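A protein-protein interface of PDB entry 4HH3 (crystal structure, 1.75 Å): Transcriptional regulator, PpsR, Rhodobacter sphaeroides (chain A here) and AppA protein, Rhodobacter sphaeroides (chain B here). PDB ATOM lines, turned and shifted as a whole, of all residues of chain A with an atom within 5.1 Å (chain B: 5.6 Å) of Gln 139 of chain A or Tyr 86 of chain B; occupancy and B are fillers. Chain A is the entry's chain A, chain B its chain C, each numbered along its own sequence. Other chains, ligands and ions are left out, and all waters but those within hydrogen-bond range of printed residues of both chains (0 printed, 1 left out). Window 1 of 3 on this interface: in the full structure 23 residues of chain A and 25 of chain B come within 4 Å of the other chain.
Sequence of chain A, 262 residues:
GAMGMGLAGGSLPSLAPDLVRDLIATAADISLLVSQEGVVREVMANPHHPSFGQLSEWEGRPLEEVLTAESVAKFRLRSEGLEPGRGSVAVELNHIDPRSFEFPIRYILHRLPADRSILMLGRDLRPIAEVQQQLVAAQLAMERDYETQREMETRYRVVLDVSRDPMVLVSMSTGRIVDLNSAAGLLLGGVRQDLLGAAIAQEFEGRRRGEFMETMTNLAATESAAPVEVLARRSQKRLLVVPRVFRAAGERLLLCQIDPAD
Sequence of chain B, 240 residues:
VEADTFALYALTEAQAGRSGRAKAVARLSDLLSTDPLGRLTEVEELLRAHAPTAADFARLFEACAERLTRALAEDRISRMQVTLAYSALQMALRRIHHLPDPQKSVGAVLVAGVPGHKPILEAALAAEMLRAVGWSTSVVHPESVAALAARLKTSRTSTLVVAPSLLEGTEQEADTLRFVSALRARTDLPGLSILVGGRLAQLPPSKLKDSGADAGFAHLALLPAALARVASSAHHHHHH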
ATOM      1  N   LEU A 135      31.022  -8.625   2.642  1.00  0.00           N
ATOM      2  CA  LEU A 135      29.825  -7.998   3.192  1.00  0.00           C
ATOM      3  C   LEU A 135      29.025  -7.295   2.084  1.00  0.00           C
ATOM      4  O   LEU A 135      27.791  -7.407   2.025  1.00  0.00           O
ATOM      5  CB  LEU A 135      30.207  -7.016   4.303  1.00  0.00           C
ATOM      6  CG  LEU A 135      29.094  -6.128   4.865  1.00  0.00           C
ATOM      7  CD1 LEU A 135      27.917  -6.973   5.354  1.00  0.00           C
ATOM      8  CD2 LEU A 135      29.628  -5.231   5.987  1.00  0.00           C
ATOM      9  N   VAL A 136      29.725  -6.584   1.203  1.00  0.00           N
ATOM     10  CA  VAL A 136      29.056  -5.920   0.071  1.00  0.00           C
ATOM     11  C   VAL A 136      28.371  -6.955  -0.834  1.00  0.00           C
ATOM     12  O   VAL A 136      27.246  -6.765  -1.289  1.00  0.00           O
ATOM     13  CB  VAL A 136      30.040  -5.067  -0.750  1.00  0.00           C
ATOM     14  CG1 VAL A 136      29.394  -4.605  -2.068  1.00  0.00           C
ATOM     15  CG2 VAL A 136      30.523  -3.872   0.074  1.00  0.00           C
ATOM     16  N   ALA A 137      29.041  -8.078  -1.058  1.00  0.00           N
ATOM     17  CA  ALA A 137      28.451  -9.152  -1.845  1.00  0.00           C
ATOM     18  C   ALA A 137      27.163  -9.685  -1.211  1.00  0.00           C
ATOM     19  O   ALA A 137      26.211 -10.026  -1.909  1.00  0.00           O
ATOM     20  CB  ALA A 137      29.469 -10.280  -2.034  1.00  0.00           C
ATOM     21  N   ALA A 138      27.141  -9.757   0.117  1.00  0.00           N
ATOM     22  CA  ALA A 138      25.976 -10.266   0.827  1.00  0.00           C
ATOM     23  C   ALA A 138      24.841  -9.251   0.787  1.00  0.00           C
ATOM     24  O   ALA A 138      23.681  -9.634   0.667  1.00  0.00           O
ATOM     25  CB  ALA A 138      26.330 -10.617   2.257  1.00  0.00           C
ATOM     26  N   GLN A 139      25.183  -7.966   0.881  1.00  0.00           N
ATOM     27  CA  GLN A 139      24.185  -6.891   0.738  1.00  0.00           C
ATOM     28  C   GLN A 139      23.488  -6.981  -0.612  1.00  0.00           C
ATOM     29  O   GLN A 139      22.272  -6.869  -0.704  1.00  0.00           O
ATOM     30  CB  GLN A 139      24.825  -5.515   0.883  1.00  0.00           C
ATOM     31  CG  GLN A 139      25.457  -5.285   2.231  1.00  0.00           C
ATOM     32  CD  GLN A 139      25.988  -3.892   2.398  1.00  0.00           C
ATOM     33  OE1 GLN A 139      27.163  -3.700   2.696  1.00  0.00           O
ATOM     34  NE2 GLN A 139      25.121  -2.905   2.221  1.00  0.00           N
ATOM     35  N   LEU A 140      24.282  -7.191  -1.653  1.00  0.00           N
ATOM     36  CA  LEU A 140      23.772  -7.362  -2.997  1.00  0.00           C
ATOM     37  C   LEU A 140      22.889  -8.609  -3.111  1.00  0.00           C
ATOM     38  O   LEU A 140      21.794  -8.559  -3.680  1.00  0.00           O
ATOM     39  CB  LEU A 140      24.943  -7.426  -3.988  1.00  0.00           C
ATOM     40  CG  LEU A 140      24.567  -7.589  -5.458  1.00  0.00           C
ATOM     41  CD1 LEU A 140      23.727  -6.400  -5.907  1.00  0.00           C
ATOM     42  CD2 LEU A 140      25.832  -7.706  -6.315  1.00  0.00           C
ATOM     43  N   ALA A 141      23.348  -9.728  -2.556  1.00  0.00           N
ATOM     44  CA  ALA A 141      22.560 -10.962  -2.609  1.00  0.00           C
ATOM     45  C   ALA A 141      21.221 -10.805  -1.896  1.00  0.00           C
ATOM     46  O   ALA A 141      20.195 -11.294  -2.371  1.00  0.00           O
ATOM     47  CB  ALA A 141      23.355 -12.143  -2.026  1.00  0.00           C
ATOM     48  N   MET A 142      21.222 -10.112  -0.764  1.00  0.00           N
ATOM     49  CA  MET A 142      19.972  -9.903  -0.015  1.00  0.00           C
ATOM     50  C   MET A 142      18.961  -9.056  -0.788  1.00  0.00           C
ATOM     51  O   MET A 142      17.769  -9.361  -0.788  1.00  0.00           O
ATOM     52  CB  MET A 142      20.237  -9.280   1.355  1.00  0.00           C
ATOM     53  CG  MET A 142      21.050 -10.159   2.319  1.00  0.00           C
ATOM     54  SD  MET A 142      20.260 -11.736   2.694  1.00  0.00           S
ATOM     55  CE  MET A 142      21.098 -12.860   1.570  1.00  0.00           C
ATOM     56  N   GLU A 143      19.436  -8.002  -1.448  1.00  0.00           N
ATOM     57  CA  GLU A 143      18.545  -7.175  -2.255  1.00  0.00           C
ATOM     58  C   GLU A 143      18.084  -7.868  -3.544  1.00  0.00           C
ATOM     59  O   GLU A 143      16.968  -7.632  -4.015  1.00  0.00           O
ATOM     60  CB  GLU A 143      19.173  -5.799  -2.521  1.00  0.00           C
ATOM     61  CG  GLU A 143      19.026  -4.862  -1.303  1.00  0.00           C
ATOM     62  CD  GLU A 143      17.562  -4.531  -1.004  1.00  0.00           C
ATOM     63  OE1 GLU A 143      17.144  -4.606   0.176  1.00  0.00           O
ATOM     64  OE2 GLU A 143      16.826  -4.197  -1.954  1.00  0.00           O
ATOM     65  N   PHE B  61      19.211  10.260   4.159  1.00  0.00           N
ATOM     66  CA  PHE B  61      20.396   9.482   3.791  1.00  0.00           C
ATOM     67  C   PHE B  61      21.392  10.341   3.018  1.00  0.00           C
ATOM     68  O   PHE B  61      22.590  10.328   3.314  1.00  0.00           O
ATOM     69  CB  PHE B  61      20.038   8.254   2.959  1.00  0.00           C
ATOM     70  CG  PHE B  61      21.231   7.635   2.261  1.00  0.00           C
ATOM     71  CD1 PHE B  61      22.322   7.194   2.988  1.00  0.00           C
ATOM     72  CD2 PHE B  61      21.255   7.506   0.883  1.00  0.00           C
ATOM     73  CE1 PHE B  61      23.438   6.639   2.348  1.00  0.00           C
ATOM     74  CE2 PHE B  61      22.358   6.946   0.236  1.00  0.00           C
ATOM     75  CZ  PHE B  61      23.444   6.511   0.972  1.00  0.00           C
ATOM     76  N   GLN B  81      34.445   1.542   8.184  1.00  0.00           N
ATOM     77  CA  GLN B  81      33.346   2.119   8.956  1.00  0.00           C
ATOM     78  C   GLN B  81      32.186   2.574   8.080  1.00  0.00           C
ATOM     79  O   GLN B  81      31.025   2.404   8.453  1.00  0.00           O
ATOM     80  CB  GLN B  81      33.849   3.275   9.830  1.00  0.00           C
ATOM     81  CG  GLN B  81      34.658   2.795  11.034  1.00  0.00           C
ATOM     82  CD  GLN B  81      35.265   3.940  11.815  1.00  0.00           C
ATOM     83  OE1 GLN B  81      36.256   4.530  11.395  1.00  0.00           O
ATOM     84  NE2 GLN B  81      34.667   4.264  12.956  1.00  0.00           N
ATOM     85  N   VAL B  82      32.490   3.144   6.916  1.00  0.00           N
ATOM     86  CA  VAL B  82      31.434   3.553   5.986  1.00  0.00           C
ATOM     87  C   VAL B  82      30.667   2.324   5.487  1.00  0.00           C
ATOM     88  O   VAL B  82      29.448   2.344   5.335  1.00  0.00           O
ATOM     89  CB  VAL B  82      32.019   4.348   4.803  1.00  0.00           C
ATOM     90  CG1 VAL B  82      30.952   4.652   3.761  1.00  0.00           C
ATOM     91  CG2 VAL B  82      32.651   5.633   5.315  1.00  0.00           C
ATOM     92  N   THR B  83      31.399   1.242   5.248  1.00  0.00           N
ATOM     93  CA  THR B  83      30.785  -0.009   4.820  1.00  0.00           C
ATOM     94  C   THR B  83      29.817  -0.555   5.870  1.00  0.00           C
ATOM     95  O   THR B  83      28.716  -1.020   5.532  1.00  0.00           O
ATOM     96  CB  THR B  83      31.861  -1.053   4.512  1.00  0.00           C
ATOM     97  OG1 THR B  83      32.712  -0.536   3.480  1.00  0.00           O
ATOM     98  CG2 THR B  83      31.238  -2.353   4.038  1.00  0.00           C
ATOM     99  N   LEU B  84      30.207  -0.488   7.138  1.00  0.00           N
ATOM    100  CA  LEU B  84      29.310  -0.932   8.209  1.00  0.00           C
ATOM    101  C   LEU B  84      28.070  -0.045   8.286  1.00  0.00           C
ATOM    102  O   LEU B  84      26.949  -0.543   8.471  1.00  0.00           O
ATOM    103  CB  LEU B  84      30.019  -0.918   9.562  1.00  0.00           C
ATOM    104  CG  LEU B  84      31.113  -1.934   9.862  1.00  0.00           C
ATOM    105  CD1 LEU B  84      31.808  -1.552  11.160  1.00  0.00           C
ATOM    106  CD2 LEU B  84      30.522  -3.339   9.977  1.00  0.00           C
ATOM    107  N   ALA B  85      28.274   1.266   8.168  1.00  0.00           N
ATOM    108  CA  ALA B  85      27.162   2.228   8.185  1.00  0.00           C
ATOM    109  C   ALA B  85      26.164   1.914   7.087  1.00  0.00           C
ATOM    110  O   ALA B  85      24.952   1.976   7.278  1.00  0.00           O
ATOM    111  CB  ALA B  85      27.682   3.642   7.991  1.00  0.00           C
ATOM    112  N   TYR B  86      26.692   1.617   5.910  1.00  0.00           N
ATOM    113  CA  TYR B  86      25.868   1.391   4.741  1.00  0.00           C
ATOM    114  C   TYR B  86      25.027   0.113   4.904  1.00  0.00           C
ATOM    115  O   TYR B  86      23.848   0.086   4.523  1.00  0.00           O
ATOM    116  CB  TYR B  86      26.795   1.329   3.541  1.00  0.00           C
ATOM    117  CG  TYR B  86      26.170   1.449   2.194  1.00  0.00           C
ATOM    118  CD1 TYR B  86      25.717   2.668   1.710  1.00  0.00           C
ATOM    119  CD2 TYR B  86      26.102   0.341   1.364  1.00  0.00           C
ATOM    120  CE1 TYR B  86      25.183   2.771   0.431  1.00  0.00           C
ATOM    121  CE2 TYR B  86      25.565   0.422   0.105  1.00  0.00           C
ATOM    122  CZ  TYR B  86      25.108   1.620  -0.357  1.00  0.00           C
ATOM    123  OH  TYR B  86      24.592   1.655  -1.628  1.00  0.00           O
ATOM    124  N   SER B  87      25.612  -0.937   5.478  1.00  0.00           N
ATOM    125  CA  SER B  87      24.861  -2.157   5.767  1.00  0.00           C
ATOM    126  C   SER B  87      23.751  -1.888   6.776  1.00  0.00           C
ATOM    127  O   SER B  87      22.632  -2.386   6.637  1.00  0.00           O
ATOM    128  CB  SER B  87      25.784  -3.260   6.298  1.00  0.00           C
ATOM    129  OG  SER B  87      26.783  -3.584   5.343  1.00  0.00           O
ATOM    130  N   ALA B  88      24.059  -1.100   7.802  1.00  0.00           N
ATOM    131  CA  ALA B  88      23.054  -0.789   8.817  1.00  0.00           C
ATOM    132  C   ALA B  88      21.892   0.015   8.227  1.00  0.00           C
ATOM    133  O   ALA B  88      20.733  -0.210   8.589  1.00  0.00           O
ATOM    134  CB  ALA B  88      23.681  -0.046   9.995  1.00  0.00           C
ATOM    135  N   LEU B  89      22.201   0.952   7.331  1.00  0.00           N
ATOM    136  CA  LEU B  89      21.154   1.728   6.649  1.00  0.00           C
ATOM    137  C   LEU B  89      20.247   0.844   5.812  1.00  0.00           C
ATOM    138  O   LEU B  89      19.032   1.044   5.766  1.00  0.00           O
ATOM    139  CB  LEU B  89      21.769   2.814   5.765  1.00  0.00           C
ATOM    140  CG  LEU B  89      22.292   4.019   6.533  1.00  0.00           C
ATOM    141  CD1 LEU B  89      23.245   4.824   5.653  1.00  0.00           C
ATOM    142  CD2 LEU B  89      21.100   4.871   6.966  1.00  0.00           C
ATOM    143  N   GLN B  90      20.843  -0.114   5.120  1.00  0.00           N
ATOM    144  CA  GLN B  90      20.087  -1.058   4.321  1.00  0.00           C
ATOM    145  C   GLN B  90      19.138  -1.865   5.204  1.00  0.00           C
ATOM    146  O   GLN B  90      17.963  -2.048   4.860  1.00  0.00           O
ATOM    147  CB  GLN B  90      21.036  -1.987   3.570  1.00  0.00           C
ATOM    148  CG  GLN B  90      20.359  -2.890   2.586  1.00  0.00           C
ATOM    149  CD  GLN B  90      21.367  -3.719   1.797  1.00  0.00           C
ATOM    150  OE1 GLN B  90      22.477  -3.257   1.508  1.00  0.00           O
ATOM    151  NE2 GLN B  90      20.994  -4.948   1.461  1.00  0.00           N
ATOM    152  N   MET B  91      19.641  -2.351   6.338  1.00  0.00           N
ATOM    153  CA  MET B  91      18.780  -3.066   7.283  1.00  0.00           C
ATOM    154  C   MET B  91      17.638  -2.169   7.787  1.00  0.00           C
ATOM    155  O   MET B  91      16.473  -2.597   7.828  1.00  0.00           O
ATOM    156  CB  MET B  91      19.602  -3.603   8.458  1.00  0.00           C
ATOM    157  CG  MET B  91      20.623  -4.681   8.061  1.00  0.00           C
ATOM    158  SD  MET B  91      21.775  -5.047   9.396  1.00  0.00           S
ATOM    159  CE  MET B  91      20.762  -6.019  10.497  1.00  0.00           C
ATOM    160  N   LYS B 118      28.413  -0.218  -6.794  1.00  0.00           N
ATOM    161  CA  LYS B 118      27.354  -0.933  -6.074  1.00  0.00           C
ATOM    162  C   LYS B 118      26.447   0.011  -5.298  1.00  0.00           C
ATOM    163  O   LYS B 118      26.506   0.067  -4.067  1.00  0.00           O
ATOM    164  CB  LYS B 118      27.973  -1.971  -5.124  1.00  0.00           C
ATOM    165  CG  LYS B 118      28.759  -3.074  -5.827  1.00  0.00           C
ATOM    166  CD  LYS B 118      27.881  -3.861  -6.788  1.00  0.00           C
ATOM    167  CE  LYS B 118      28.638  -5.018  -7.418  1.00  0.00           C
ATOM    168  NZ  LYS B 118      27.915  -5.560  -8.605  1.00  0.00           N
ATOM    169  N   PRO B 119      25.586   0.765  -6.011  1.00  0.00           N
ATOM    170  CA  PRO B 119      24.653   1.666  -5.340  1.00  0.00           C
ATOM    171  C   PRO B 119      23.445   0.882  -4.834  1.00  0.00           C
ATOM    172  O   PRO B 119      22.318   1.095  -5.267  1.00  0.00           O
ATOM    173  CB  PRO B 119      24.250   2.636  -6.452  1.00  0.00           C
ATOM    174  CG  PRO B 119      24.340   1.807  -7.695  1.00  0.00           C
ATOM    175  CD  PRO B 119      25.445   0.807  -7.475  1.00  0.00           C
ATOM    176  N   ILE B 120      23.693  -0.040  -3.913  1.00  0.00           N
ATOM    177  CA  ILE B 120      22.624  -0.947  -3.472  1.00  0.00           C
ATOM    178  C   ILE B 120      21.518  -0.193  -2.747  1.00  0.00           C
ATOM    179  O   ILE B 120      20.326  -0.398  -3.021  1.00  0.00           O
ATOM    180  CB  ILE B 120      23.204  -2.049  -2.558  1.00  0.00           C
ATOM    181  CG1 ILE B 120      24.275  -2.826  -3.319  1.00  0.00           C
ATOM    182  CG2 ILE B 120      22.073  -2.997  -2.054  1.00  0.00           C
ATOM    183  CD1 ILE B 120      25.172  -3.686  -2.445  1.00  0.00           C
ATOM    184  N   LEU B 121      21.903   0.659  -1.795  1.00  0.00           N
ATOM    185  CA  LEU B 121      20.919   1.423  -1.041  1.00  0.00           C
ATOM    186  C   LEU B 121      20.211   2.458  -1.917  1.00  0.00           C
ATOM    187  O   LEU B 121      18.988   2.632  -1.824  1.00  0.00           O
ATOM    188  CB  LEU B 121      21.564   2.095   0.174  1.00  0.00           C
ATOM    189  CG  LEU B 121      20.610   2.893   1.066  1.00  0.00           C
ATOM    190  CD1 LEU B 121      19.658   1.947   1.767  1.00  0.00           C
ATOM    191  CD2 LEU B 121      21.401   3.687   2.093  1.00  0.00           C
ATOM    192  N   GLU B 122      20.975   3.135  -2.777  1.00  0.00           N
ATOM    193  CA  GLU B 122      20.400   4.176  -3.636  1.00  0.00           C
ATOM    194  C   GLU B 122      19.408   3.614  -4.641  1.00  0.00           C
ATOM    195  O   GLU B 122      18.366   4.224  -4.913  1.00  0.00           O
ATOM    196  CB  GLU B 122      21.519   4.918  -4.371  1.00  0.00           C
ATOM    197  CG  GLU B 122      22.423   5.714  -3.409  1.00  0.00           C
ATOM    198  CD  GLU B 122      23.645   4.927  -2.944  1.00  0.00           C
ATOM    199  OE1 GLU B 122      23.637   3.662  -2.982  1.00  0.00           O
ATOM    200  OE2 GLU B 122      24.631   5.582  -2.532  1.00  0.00           O
ATOM    201  N   LEU B 167      28.298   7.309  -1.828  1.00  0.00           N
ATOM    202  CA  LEU B 167      29.448   7.091  -0.948  1.00  0.00           C
ATOM    203  C   LEU B 167      30.649   6.542  -1.704  1.00  0.00           C
ATOM    204  O   LEU B 167      31.578   6.007  -1.100  1.00  0.00           O
ATOM    205  CB  LEU B 167      29.068   6.154   0.209  1.00  0.00           C
ATOM    206  CG  LEU B 167      28.143   6.812   1.242  1.00  0.00           C
ATOM    207  CD1 LEU B 167      27.524   5.787   2.181  1.00  0.00           C
ATOM    208  CD2 LEU B 167      28.948   7.862   2.027  1.00  0.00           C
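The side-chain amide oxygen (OE1) of Gln 139 of chain A sits at hydrogen-bond distance from the side-chain hydroxyl (OG) of Ser 87 of chain B, at 2.7 Å. The side-chain amide oxygen (OE1) of Gln 90 of chain B is in hydrogen-bond range of the side-chain amide nitrogen (NE2) of Gln 139 of chain A.
The side-chain hydroxyl (OH) of Tyr 86 of chain B is in hydrogen-bond range of the backbone NH (N) of Ile 120 of chain B. The side-chain hydroxyl of Tyr 86 of chain B is in hydrogen-bond range of the backbone carbonyl oxygen of Lys 118 of chain B (3.5 Å). The backbone NH (N) of Leu 121 of chain B sits at hydrogen-bond distance from the side-chain hydroxyl (OH) of Tyr 86 of chain B. The side-chain hydroxyl (OG) of Ser 87 of chain B is in hydrogen-bond range of the backbone carbonyl oxygen (O) of Thr 83 of chain B (3.2 Å). OH of Tyr 86 of chain B is in hydrogen-bond range of OE1 of Glu 122 of chain B.
Thr 83 of chain B touches Leu 135 of chain A (CG2 to CD2, 3.8 Å). Leu 135 of chain A touches Ser 87 of chain B (CD2 to OG, 3.3 Å). O of Val 136 of chain A touches CD1 of Ile 120 of chain B, at 3.9 Å. Tyr 86 of chain B touches Gln 139 of chain A (CD2 to NE2, 3.5 Å). Gln 139 of chain A touches Ile 120 of chain B. Lys 118 of chain B touches Leu 140 of chain A (NZ to CD2, 3.8 Å). Ile 120 of chain B touches Leu 140 of chain A (CD1 to N, 3.7 Å). Glu 143 of chain A touches Gln 90 of chain B (CG to NE2, 3.4 Å). CG2 of Ile 120 of chain B touches CG of Glu 143 of chain A, at 3.7 Å.
Printed residues of chain B within 4 Å of Gln 139 of chain A: Tyr 86 (3.5 Å), Ser 87 (2.7 Å), Gln 90 (2.8 Å) and Ile 120 (3.8 Å). Of chain A, only Gln 139 comes within 4 Å of Tyr 86 of chain B. Of the printed residues of chain A, Thr 83 of chain B touches Leu 135. Of the printed residues of chain B, Leu 140 of chain A touches Lys 118 and Ile 120. Ala 85 of chain B touches none of the printed residues of chain A. Leu 89 of chain B touches none of the printed residues of chain A. The nearest printed residue of chain B that does not touch Gln 139 of chain A is Thr 83 of chain B (4.2 Å). The nearest printed residue of chain A that does not touch Tyr 86 of chain B is Val 136 of chain A (6.2 Å). The nearest printed residue of chain B that does not touch Glu 143 of chain A is Leu 121 of chain B (6.2 Å).
Hydrophobic or aromatic side chains of chain B within 4 Å of the printed part of chain A: Tyr 86 and Ile 120. Among the printed residues, 11 pairs touch across the chains.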
